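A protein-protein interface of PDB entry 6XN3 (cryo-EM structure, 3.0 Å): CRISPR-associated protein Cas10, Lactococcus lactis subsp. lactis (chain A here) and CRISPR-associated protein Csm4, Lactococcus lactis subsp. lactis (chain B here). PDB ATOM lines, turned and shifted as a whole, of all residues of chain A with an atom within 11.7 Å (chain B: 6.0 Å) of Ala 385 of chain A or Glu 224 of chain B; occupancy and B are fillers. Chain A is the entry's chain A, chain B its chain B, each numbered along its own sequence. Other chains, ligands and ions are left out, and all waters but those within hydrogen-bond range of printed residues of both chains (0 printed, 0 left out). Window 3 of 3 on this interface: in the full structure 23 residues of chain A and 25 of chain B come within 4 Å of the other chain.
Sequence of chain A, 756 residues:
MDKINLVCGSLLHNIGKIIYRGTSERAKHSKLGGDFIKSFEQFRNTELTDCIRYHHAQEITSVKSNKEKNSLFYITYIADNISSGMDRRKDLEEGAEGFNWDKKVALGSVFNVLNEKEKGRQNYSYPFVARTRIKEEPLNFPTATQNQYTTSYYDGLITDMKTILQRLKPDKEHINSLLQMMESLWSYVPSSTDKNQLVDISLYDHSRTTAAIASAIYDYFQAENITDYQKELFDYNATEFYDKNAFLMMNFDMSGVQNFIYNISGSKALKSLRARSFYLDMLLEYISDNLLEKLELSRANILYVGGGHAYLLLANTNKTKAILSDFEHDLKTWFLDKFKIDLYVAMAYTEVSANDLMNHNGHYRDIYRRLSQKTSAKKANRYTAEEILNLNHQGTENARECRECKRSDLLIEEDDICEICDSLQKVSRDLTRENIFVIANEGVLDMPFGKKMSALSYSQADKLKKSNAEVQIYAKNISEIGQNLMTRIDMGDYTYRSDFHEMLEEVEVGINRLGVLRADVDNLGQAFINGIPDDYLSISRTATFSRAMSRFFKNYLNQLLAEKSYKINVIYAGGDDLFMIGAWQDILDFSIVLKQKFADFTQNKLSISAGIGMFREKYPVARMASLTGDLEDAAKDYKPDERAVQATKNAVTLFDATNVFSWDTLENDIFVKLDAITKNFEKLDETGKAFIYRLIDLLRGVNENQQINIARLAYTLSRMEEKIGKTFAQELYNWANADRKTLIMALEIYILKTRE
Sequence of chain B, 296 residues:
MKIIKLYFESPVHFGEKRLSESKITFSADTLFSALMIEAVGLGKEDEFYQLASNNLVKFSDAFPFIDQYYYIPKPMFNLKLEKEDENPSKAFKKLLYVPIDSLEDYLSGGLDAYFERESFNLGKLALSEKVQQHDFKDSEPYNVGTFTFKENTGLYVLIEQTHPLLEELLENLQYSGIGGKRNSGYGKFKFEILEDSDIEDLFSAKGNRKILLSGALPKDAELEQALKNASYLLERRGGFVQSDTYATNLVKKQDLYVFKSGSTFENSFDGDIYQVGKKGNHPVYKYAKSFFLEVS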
ATOM      1  N   HIS A 329      11.452 -28.279 -18.344  1.00  0.00           N
ATOM      2  CA  HIS A 329      10.804 -26.973 -18.422  1.00  0.00           C
ATOM      3  C   HIS A 329      11.079 -26.147 -17.171  1.00  0.00           C
ATOM      4  O   HIS A 329      11.408 -24.955 -17.259  1.00  0.00           O
ATOM      5  CB  HIS A 329       9.305 -27.141 -18.646  1.00  0.00           C
ATOM      6  CG  HIS A 329       8.552 -25.851 -18.650  1.00  0.00           C
ATOM      7  ND1 HIS A 329       7.622 -25.529 -17.688  1.00  0.00           N
ATOM      8  CD2 HIS A 329       8.594 -24.800 -19.501  1.00  0.00           C
ATOM      9  CE1 HIS A 329       7.122 -24.333 -17.945  1.00  0.00           C
ATOM     10  NE2 HIS A 329       7.696 -23.868 -19.041  1.00  0.00           N
ATOM     11  N   LYS A 332      14.991 -25.175 -17.056  1.00  0.00           N
ATOM     12  CA  LYS A 332      15.269 -24.186 -18.087  1.00  0.00           C
ATOM     13  C   LYS A 332      14.702 -22.826 -17.716  1.00  0.00           C
ATOM     14  O   LYS A 332      15.388 -21.806 -17.854  1.00  0.00           O
ATOM     15  CB  LYS A 332      14.695 -24.673 -19.413  1.00  0.00           C
ATOM     16  CG  LYS A 332      15.040 -23.827 -20.601  1.00  0.00           C
ATOM     17  CD  LYS A 332      14.152 -24.191 -21.767  1.00  0.00           C
ATOM     18  CE  LYS A 332      14.608 -25.491 -22.396  1.00  0.00           C
ATOM     19  NZ  LYS A 332      15.805 -25.304 -23.256  1.00  0.00           N
ATOM     20  N   THR A 333      13.469 -22.793 -17.195  1.00  0.00           N
ATOM     21  CA  THR A 333      12.880 -21.522 -16.788  1.00  0.00           C
ATOM     22  C   THR A 333      13.606 -20.930 -15.589  1.00  0.00           C
ATOM     23  O   THR A 333      13.719 -19.703 -15.472  1.00  0.00           O
ATOM     24  CB  THR A 333      11.398 -21.701 -16.474  1.00  0.00           C
ATOM     25  OG1 THR A 333      10.668 -21.872 -17.692  1.00  0.00           O
ATOM     26  N   LEU A 336      16.744 -19.379 -16.864  1.00  0.00           N
ATOM     27  CA  LEU A 336      16.457 -18.195 -17.666  1.00  0.00           C
ATOM     28  C   LEU A 336      15.960 -17.038 -16.809  1.00  0.00           C
ATOM     29  O   LEU A 336      16.025 -15.881 -17.236  1.00  0.00           O
ATOM     30  CB  LEU A 336      15.443 -18.532 -18.750  1.00  0.00           C
ATOM     31  CG  LEU A 336      16.055 -19.297 -19.918  1.00  0.00           C
ATOM     32  CD1 LEU A 336      14.990 -20.021 -20.706  1.00  0.00           C
ATOM     33  CD2 LEU A 336      16.842 -18.397 -20.801  1.00  0.00           C
ATOM     34  N   TYR A 344      23.460 -22.830 -18.850  1.00  0.00           N
ATOM     35  CA  TYR A 344      22.471 -23.678 -19.489  1.00  0.00           C
ATOM     36  C   TYR A 344      22.858 -25.135 -19.309  1.00  0.00           C
ATOM     37  O   TYR A 344      23.988 -25.522 -19.611  1.00  0.00           O
ATOM     38  CB  TYR A 344      22.346 -23.360 -20.977  1.00  0.00           C
ATOM     39  CG  TYR A 344      21.208 -24.088 -21.624  1.00  0.00           C
ATOM     40  CD1 TYR A 344      19.942 -24.056 -21.062  1.00  0.00           C
ATOM     41  CD2 TYR A 344      21.394 -24.805 -22.792  1.00  0.00           C
ATOM     42  CE1 TYR A 344      18.891 -24.715 -21.642  1.00  0.00           C
ATOM     43  CE2 TYR A 344      20.349 -25.472 -23.382  1.00  0.00           C
ATOM     44  CZ  TYR A 344      19.099 -25.421 -22.802  1.00  0.00           C
ATOM     45  OH  TYR A 344      18.048 -26.084 -23.382  1.00  0.00           O
ATOM     46  N   ALA A 380      22.679 -26.753 -29.729  1.00  0.00           N
ATOM     47  CA  ALA A 380      22.607 -25.922 -30.925  1.00  0.00           C
ATOM     48  C   ALA A 380      21.314 -25.123 -30.970  1.00  0.00           C
ATOM     49  O   ALA A 380      21.296 -23.986 -31.449  1.00  0.00           O
ATOM     50  CB  ALA A 380      22.748 -26.788 -32.173  1.00  0.00           C
ATOM     51  N   ASN A 381      20.220 -25.704 -30.486  1.00  0.00           N
ATOM     52  CA  ASN A 381      18.905 -25.070 -30.474  1.00  0.00           C
ATOM     53  C   ASN A 381      18.472 -24.994 -29.015  1.00  0.00           C
ATOM     54  O   ASN A 381      17.756 -25.857 -28.514  1.00  0.00           O
ATOM     55  CB  ASN A 381      17.920 -25.887 -31.335  1.00  0.00           C
ATOM     56  CG  ASN A 381      16.545 -25.251 -31.445  1.00  0.00           C
ATOM     57  OD1 ASN A 381      16.299 -24.153 -30.955  1.00  0.00           O
ATOM     58  ND2 ASN A 381      15.631 -25.961 -32.091  1.00  0.00           N
ATOM     59  N   ARG A 382      18.892 -23.929 -28.335  1.00  0.00           N
ATOM     60  CA  ARG A 382      18.747 -23.890 -26.884  1.00  0.00           C
ATOM     61  C   ARG A 382      17.331 -23.523 -26.472  1.00  0.00           C
ATOM     62  O   ARG A 382      16.625 -24.320 -25.849  1.00  0.00           O
ATOM     63  CB  ARG A 382      19.746 -22.908 -26.276  1.00  0.00           C
ATOM     64  CG  ARG A 382      21.165 -23.411 -26.276  1.00  0.00           C
ATOM     65  CD  ARG A 382      22.089 -22.481 -25.536  1.00  0.00           C
ATOM     66  NE  ARG A 382      23.464 -22.958 -25.577  1.00  0.00           N
ATOM     67  CZ  ARG A 382      24.478 -22.341 -24.989  1.00  0.00           C
ATOM     68  NH1 ARG A 382      24.265 -21.228 -24.307  1.00  0.00           N
ATOM     69  NH2 ARG A 382      25.700 -22.840 -25.079  1.00  0.00           N
ATOM     70  N   TYR A 383      16.893 -22.324 -26.810  1.00  0.00           N
ATOM     71  CA  TYR A 383      15.655 -21.803 -26.267  1.00  0.00           C
ATOM     72  C   TYR A 383      14.571 -21.847 -27.329  1.00  0.00           C
ATOM     73  O   TYR A 383      14.846 -21.787 -28.528  1.00  0.00           O
ATOM     74  CB  TYR A 383      15.853 -20.375 -25.759  1.00  0.00           C
ATOM     75  CG  TYR A 383      17.168 -20.187 -25.045  1.00  0.00           C
ATOM     76  CD1 TYR A 383      17.418 -20.809 -23.834  1.00  0.00           C
ATOM     77  CD2 TYR A 383      18.162 -19.393 -25.589  1.00  0.00           C
ATOM     78  CE1 TYR A 383      18.619 -20.643 -23.187  1.00  0.00           C
ATOM     79  CE2 TYR A 383      19.365 -19.222 -24.949  1.00  0.00           C
ATOM     80  CZ  TYR A 383      19.587 -19.848 -23.748  1.00  0.00           C
ATOM     81  OH  TYR A 383      20.786 -19.682 -23.103  1.00  0.00           O
ATOM     82  N   THR A 384      13.327 -21.958 -26.879  1.00  0.00           N
ATOM     83  CA  THR A 384      12.209 -21.978 -27.803  1.00  0.00           C
ATOM     84  C   THR A 384      11.806 -20.549 -28.150  1.00  0.00           C
ATOM     85  O   THR A 384      12.498 -19.584 -27.821  1.00  0.00           O
ATOM     86  CB  THR A 384      11.034 -22.753 -27.220  1.00  0.00           C
ATOM     87  OG1 THR A 384      10.315 -21.915 -26.313  1.00  0.00           O
ATOM     88  N   ALA A 385      10.673 -20.409 -28.832  1.00  0.00           N
ATOM     89  CA  ALA A 385      10.281 -19.107 -29.349  1.00  0.00           C
ATOM     90  C   ALA A 385       9.823 -18.163 -28.252  1.00  0.00           C
ATOM     91  O   ALA A 385      10.268 -17.010 -28.198  1.00  0.00           O
ATOM     92  CB  ALA A 385       9.180 -19.269 -30.391  1.00  0.00           C
ATOM     93  N   GLU A 386       8.953 -18.634 -27.358  1.00  0.00           N
ATOM     94  CA  GLU A 386       8.419 -17.746 -26.333  1.00  0.00           C
ATOM     95  C   GLU A 386       9.460 -17.427 -25.274  1.00  0.00           C
ATOM     96  O   GLU A 386       9.364 -16.385 -24.622  1.00  0.00           O
ATOM     97  CB  GLU A 386       7.161 -18.340 -25.685  1.00  0.00           C
ATOM     98  CG  GLU A 386       7.302 -19.679 -24.949  1.00  0.00           C
ATOM     99  CD  GLU A 386       7.386 -20.912 -25.848  1.00  0.00           C
ATOM    100  OE1 GLU A 386       7.650 -20.794 -27.066  1.00  0.00           O
ATOM    101  OE2 GLU A 386       7.176 -22.024 -25.317  1.00  0.00           O
ATOM    102  N   GLU A 387      10.476 -18.279 -25.120  1.00  0.00           N
ATOM    103  CA  GLU A 387      11.568 -17.971 -24.205  1.00  0.00           C
ATOM    104  C   GLU A 387      12.394 -16.797 -24.714  1.00  0.00           C
ATOM    105  O   GLU A 387      12.720 -15.884 -23.950  1.00  0.00           O
ATOM    106  CB  GLU A 387      12.445 -19.200 -23.998  1.00  0.00           C
ATOM    107  CG  GLU A 387      11.655 -20.467 -23.736  1.00  0.00           C
ATOM    108  CD  GLU A 387      11.081 -20.537 -22.335  1.00  0.00           C
ATOM    109  OE1 GLU A 387       9.855 -20.362 -22.184  1.00  0.00           O
ATOM    110  OE2 GLU A 387      11.851 -20.779 -21.385  1.00  0.00           O
ATOM    111  N   ILE A 388      12.704 -16.784 -26.014  1.00  0.00           N
ATOM    112  CA  ILE A 388      13.429 -15.660 -26.609  1.00  0.00           C
ATOM    113  C   ILE A 388      12.565 -14.405 -26.602  1.00  0.00           C
ATOM    114  O   ILE A 388      13.054 -13.300 -26.329  1.00  0.00           O
ATOM    115  CB  ILE A 388      13.900 -16.025 -28.029  1.00  0.00           C
ATOM    116  CG1 ILE A 388      14.940 -17.134 -27.976  1.00  0.00           C
ATOM    117  CG2 ILE A 388      14.522 -14.848 -28.738  1.00  0.00           C
ATOM    118  CD1 ILE A 388      15.224 -17.741 -29.319  1.00  0.00           C
ATOM    119  N   LEU A 389      11.264 -14.559 -26.862  1.00  0.00           N
ATOM    120  CA  LEU A 389      10.358 -13.412 -26.868  1.00  0.00           C
ATOM    121  C   LEU A 389      10.231 -12.782 -25.484  1.00  0.00           C
ATOM    122  O   LEU A 389      10.304 -11.555 -25.340  1.00  0.00           O
ATOM    123  CB  LEU A 389       8.989 -13.839 -27.387  1.00  0.00           C
ATOM    124  CG  LEU A 389       8.907 -14.084 -28.888  1.00  0.00           C
ATOM    125  CD1 LEU A 389       7.667 -14.896 -29.218  1.00  0.00           C
ATOM    126  CD2 LEU A 389       8.909 -12.764 -29.621  1.00  0.00           C
ATOM    127  N   ASN A 390      10.061 -13.611 -24.448  1.00  0.00           N
ATOM    128  CA  ASN A 390      10.014 -13.108 -23.079  1.00  0.00           C
ATOM    129  C   ASN A 390      11.353 -12.522 -22.668  1.00  0.00           C
ATOM    130  O   ASN A 390      11.410 -11.492 -21.986  1.00  0.00           O
ATOM    131  CB  ASN A 390       9.618 -14.237 -22.131  1.00  0.00           C
ATOM    132  CG  ASN A 390       9.063 -13.729 -20.825  1.00  0.00           C
ATOM    133  OD1 ASN A 390       8.557 -12.613 -20.747  1.00  0.00           O
ATOM    134  ND2 ASN A 390       9.154 -14.546 -19.785  1.00  0.00           N
ATOM    135  N   LEU A 391      12.439 -13.148 -23.111  1.00  0.00           N
ATOM    136  CA  LEU A 391      13.780 -12.719 -22.750  1.00  0.00           C
ATOM    137  C   LEU A 391      14.139 -11.382 -23.383  1.00  0.00           C
ATOM    138  O   LEU A 391      14.961 -10.637 -22.841  1.00  0.00           O
ATOM    139  CB  LEU A 391      14.739 -13.837 -23.145  1.00  0.00           C
ATOM    140  CG  LEU A 391      16.224 -13.880 -22.875  1.00  0.00           C
ATOM    141  CD1 LEU A 391      16.661 -15.281 -22.698  1.00  0.00           C
ATOM    142  CD2 LEU A 391      16.772 -13.482 -24.161  1.00  0.00           C
ATOM    143  N   ASN A 392      13.547 -11.063 -24.529  1.00  0.00           N
ATOM    144  CA  ASN A 392      13.735  -9.728 -25.087  1.00  0.00           C
ATOM    145  C   ASN A 392      12.741  -8.729 -24.510  1.00  0.00           C
ATOM    146  O   ASN A 392      13.052  -7.541 -24.403  1.00  0.00           O
ATOM    147  CB  ASN A 392      13.621  -9.765 -26.606  1.00  0.00           C
ATOM    148  CG  ASN A 392      14.939 -10.036 -27.274  1.00  0.00           C
ATOM    149  OD1 ASN A 392      15.933  -9.370 -27.001  1.00  0.00           O
ATOM    150  ND2 ASN A 392      14.967 -11.030 -28.142  1.00  0.00           N
ATOM    151  N   HIS A 393      11.544  -9.184 -24.140  1.00  0.00           N
ATOM    152  CA  HIS A 393      10.545  -8.256 -23.625  1.00  0.00           C
ATOM    153  C   HIS A 393      10.830  -7.811 -22.200  1.00  0.00           C
ATOM    154  O   HIS A 393      10.393  -6.725 -21.811  1.00  0.00           O
ATOM    155  CB  HIS A 393       9.157  -8.882 -23.701  1.00  0.00           C
ATOM    156  CG  HIS A 393       8.043  -7.895 -23.562  1.00  0.00           C
ATOM    157  ND1 HIS A 393       7.707  -7.313 -22.359  1.00  0.00           N
ATOM    158  CD2 HIS A 393       7.194  -7.376 -24.481  1.00  0.00           C
ATOM    159  CE1 HIS A 393       6.695  -6.484 -22.540  1.00  0.00           C
ATOM    160  NE2 HIS A 393       6.364  -6.505 -23.818  1.00  0.00           N
ATOM    161  N   GLN A 394      11.553  -8.604 -21.411  1.00  0.00           N
ATOM    162  CA  GLN A 394      11.872  -8.201 -20.046  1.00  0.00           C
ATOM    163  C   GLN A 394      13.045  -7.231 -19.960  1.00  0.00           C
ATOM    164  O   GLN A 394      13.569  -7.016 -18.863  1.00  0.00           O
ATOM    165  CB  GLN A 394      12.160  -9.428 -19.176  1.00  0.00           C
ATOM    166  CG  GLN A 394      10.975 -10.358 -18.991  1.00  0.00           C
ATOM    167  CD  GLN A 394      10.212 -10.107 -17.707  1.00  0.00           C
ATOM    168  OE1 GLN A 394      10.123  -8.978 -17.232  1.00  0.00           O
ATOM    169  NE2 GLN A 394       9.649 -11.167 -17.139  1.00  0.00           N
ATOM    170  N   LYS B 219      11.517 -10.468 -36.536  1.00  0.00           N
ATOM    171  CA  LYS B 219      10.365  -9.811 -35.946  1.00  0.00           C
ATOM    172  C   LYS B 219       9.502 -10.832 -35.213  1.00  0.00           C
ATOM    173  O   LYS B 219       9.615 -12.041 -35.426  1.00  0.00           O
ATOM    174  CB  LYS B 219       9.545  -9.104 -37.019  1.00  0.00           C
ATOM    175  CG  LYS B 219      10.257  -7.964 -37.716  1.00  0.00           C
ATOM    176  CD  LYS B 219       9.334  -7.333 -38.741  1.00  0.00           C
ATOM    177  CE  LYS B 219       9.960  -6.124 -39.394  1.00  0.00           C
ATOM    178  NZ  LYS B 219      11.094  -6.509 -40.272  1.00  0.00           N
ATOM    179  N   ASP B 220       8.621 -10.323 -34.344  1.00  0.00           N
ATOM    180  CA  ASP B 220       7.889 -11.164 -33.401  1.00  0.00           C
ATOM    181  C   ASP B 220       6.933 -12.137 -34.076  1.00  0.00           C
ATOM    182  O   ASP B 220       6.656 -13.200 -33.513  1.00  0.00           O
ATOM    183  CB  ASP B 220       7.103 -10.299 -32.419  1.00  0.00           C
ATOM    184  CG  ASP B 220       7.995  -9.485 -31.518  1.00  0.00           C
ATOM    185  OD1 ASP B 220       9.157  -9.889 -31.319  1.00  0.00           O
ATOM    186  OD2 ASP B 220       7.534  -8.447 -31.001  1.00  0.00           O
ATOM    187  N   ALA B 221       6.433 -11.811 -35.260  1.00  0.00           N
ATOM    188  CA  ALA B 221       5.467 -12.659 -35.937  1.00  0.00           C
ATOM    189  C   ALA B 221       6.116 -13.656 -36.882  1.00  0.00           C
ATOM    190  O   ALA B 221       5.404 -14.388 -37.572  1.00  0.00           O
ATOM    191  CB  ALA B 221       4.458 -11.801 -36.702  1.00  0.00           C
ATOM    192  N   GLU B 222       7.443 -13.703 -36.934  1.00  0.00           N
ATOM    193  CA  GLU B 222       8.134 -14.628 -37.813  1.00  0.00           C
ATOM    194  C   GLU B 222       9.278 -15.359 -37.134  1.00  0.00           C
ATOM    195  O   GLU B 222      10.034 -16.059 -37.816  1.00  0.00           O
ATOM    196  CB  GLU B 222       8.669 -13.895 -39.046  1.00  0.00           C
ATOM    197  CG  GLU B 222       9.594 -12.757 -38.711  1.00  0.00           C
ATOM    198  CD  GLU B 222       9.851 -11.869 -39.900  1.00  0.00           C
ATOM    199  OE1 GLU B 222       9.346 -12.189 -40.996  1.00  0.00           O
ATOM    200  OE2 GLU B 222      10.544 -10.846 -39.738  1.00  0.00           O
ATOM    201  N   LEU B 223       9.424 -15.223 -35.814  1.00  0.00           N
ATOM    202  CA  LEU B 223      10.503 -15.907 -35.112  1.00  0.00           C
ATOM    203  C   LEU B 223      10.257 -17.406 -35.091  1.00  0.00           C
ATOM    204  O   LEU B 223      11.206 -18.198 -35.124  1.00  0.00           O
ATOM    205  CB  LEU B 223      10.631 -15.341 -33.694  1.00  0.00           C
ATOM    206  CG  LEU B 223      11.824 -15.651 -32.777  1.00  0.00           C
ATOM    207  CD1 LEU B 223      12.018 -14.498 -31.810  1.00  0.00           C
ATOM    208  CD2 LEU B 223      11.680 -16.932 -31.996  1.00  0.00           C
ATOM    209  N   GLU B 224       8.989 -17.812 -35.047  1.00  0.00           N
ATOM    210  CA  GLU B 224       8.650 -19.230 -35.076  1.00  0.00           C
ATOM    211  C   GLU B 224       8.987 -19.855 -36.423  1.00  0.00           C
ATOM    212  O   GLU B 224       9.546 -20.954 -36.487  1.00  0.00           O
ATOM    213  CB  GLU B 224       7.169 -19.417 -34.742  1.00  0.00           C
ATOM    214  CG  GLU B 224       6.694 -20.862 -34.777  1.00  0.00           C
ATOM    215  CD  GLU B 224       7.332 -21.737 -33.718  1.00  0.00           C
ATOM    216  OE1 GLU B 224       7.733 -21.221 -32.656  1.00  0.00           O
ATOM    217  OE2 GLU B 224       7.443 -22.955 -33.957  1.00  0.00           O
ATOM    218  N   GLN B 225       8.659 -19.162 -37.515  1.00  0.00           N
ATOM    219  CA  GLN B 225       8.980 -19.687 -38.835  1.00  0.00           C
ATOM    220  C   GLN B 225      10.477 -19.614 -39.098  1.00  0.00           C
ATOM    221  O   GLN B 225      11.015 -20.435 -39.845  1.00  0.00           O
ATOM    222  CB  GLN B 225       8.182 -18.923 -39.897  1.00  0.00           C
ATOM    223  CG  GLN B 225       8.243 -19.459 -41.331  1.00  0.00           C
ATOM    224  CD  GLN B 225       9.434 -18.946 -42.114  1.00  0.00           C
ATOM    225  OE1 GLN B 225       9.918 -17.843 -41.868  1.00  0.00           O
ATOM    226  NE2 GLN B 225       9.909 -19.741 -43.063  1.00  0.00           N
ATOM    227  N   ALA B 226      11.166 -18.661 -38.471  1.00  0.00           N
ATOM    228  CA  ALA B 226      12.617 -18.607 -38.572  1.00  0.00           C
ATOM    229  C   ALA B 226      13.266 -19.703 -37.744  1.00  0.00           C
ATOM    230  O   ALA B 226      14.410 -20.094 -37.999  1.00  0.00           O
ATOM    231  CB  ALA B 226      13.117 -17.238 -38.123  1.00  0.00           C
ATOM    232  N   LEU B 227      12.555 -20.205 -36.742  1.00  0.00           N
ATOM    233  CA  LEU B 227      13.117 -21.152 -35.787  1.00  0.00           C
ATOM    234  C   LEU B 227      12.494 -22.517 -36.042  1.00  0.00           C
ATOM    235  O   LEU B 227      11.486 -22.891 -35.443  1.00  0.00           O
ATOM    236  CB  LEU B 227      12.864 -20.657 -34.373  1.00  0.00           C
ATOM    237  CG  LEU B 227      13.454 -21.469 -33.242  1.00  0.00           C
ATOM    238  CD1 LEU B 227      14.914 -21.415 -33.454  1.00  0.00           C
ATOM    239  CD2 LEU B 227      13.082 -20.847 -31.915  1.00  0.00           C
ATOM    240  N   LYS B 228      13.087 -23.264 -36.965  1.00  0.00           N
ATOM    241  CA  LYS B 228      12.603 -24.595 -37.300  1.00  0.00           C
ATOM    242  C   LYS B 228      13.659 -25.664 -37.096  1.00  0.00           C
ATOM    243  O   LYS B 228      13.440 -26.613 -36.338  1.00  0.00           O
ATOM    244  CB  LYS B 228      12.117 -24.620 -38.757  1.00  0.00           C
ATOM    245  CG  LYS B 228      11.665 -25.986 -39.262  1.00  0.00           C
ATOM    246  CD  LYS B 228      10.518 -26.546 -38.444  1.00  0.00           C
ATOM    247  CE  LYS B 228       9.254 -25.726 -38.632  1.00  0.00           C
ATOM    248  NZ  LYS B 228       8.168 -26.193 -37.734  1.00  0.00           N
ATOM    249  N   ASN B 267      15.446 -21.848 -43.282  1.00  0.00           N
ATOM    250  CA  ASN B 267      14.557 -20.894 -43.922  1.00  0.00           C
ATOM    251  C   ASN B 267      14.905 -19.475 -43.498  1.00  0.00           C
ATOM    252  O   ASN B 267      15.341 -19.232 -42.371  1.00  0.00           O
ATOM    253  CB  ASN B 267      13.096 -21.225 -43.619  1.00  0.00           C
ATOM    254  CG  ASN B 267      12.847 -21.479 -42.153  1.00  0.00           C
ATOM    255  OD1 ASN B 267      13.728 -21.315 -41.317  1.00  0.00           O
ATOM    256  ND2 ASN B 267      11.638 -21.912 -41.834  1.00  0.00           N
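The backbone carbonyl oxygen (O) of Ile 388 of chain A lies within hydrogen-bond range of the side-chain amide nitrogen (ND2) of Asn 392 of chain A, at 3.5 Å.
The side-chain hydroxyl (OG1) of Thr 384 of chain A lies within hydrogen-bond range of the side-chain carboxylate (OE1) of Glu 386 of chain A.
OD1 of Asn 381 of chain A touches CD1 of Leu 227 of chain B (3.96 Å).
O of Tyr 383 of chain A touches CD2 of Leu 227 of chain B (3.9 Å).
CD2 of Leu 227 of chain B touches C of Thr 384 of chain A, 3.99 Å away.
CA of Ala 385 of chain A touches CD2 of Leu 223 of chain B, at 3.7 Å.
Ala 385 of chain A touches Glu 224 of chain B (CB to OE1, 3.3 Å).
Ala 385 of chain A touches Leu 227 of chain B (N to CD2, 3.9 Å).
Leu 223 of chain B touches Ile 388 of chain A (CD1 to CG2, 3.98 Å).
Leu 389 of chain A touches Asp 220 of chain B.
Of the printed residues of chain B, Tyr 383 of chain A touches Leu 227 (3.9 Å).
Of the printed residues of chain B, Leu 389 of chain A touches Asp 220 (3.3 Å).
Of the printed residues of chain A, Asp 220 of chain B touches Leu 389.
Of chain A, only Ala 385 (3.7 Å) and Ile 388 (3.98 Å) come within 4 Å of Leu 223 of chain B.
Of chain A, only Ala 385 comes within 4 Å of Glu 224 of chain B.
No residue of chain A comes within 4 Å of Lys 228 of chain B.
The nearest residue of chain A that does not touch Glu 224 of chain B is Glu 386 of chain A (5.6 Å).
Among the printed residues, 8 pairs touch across the chains.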
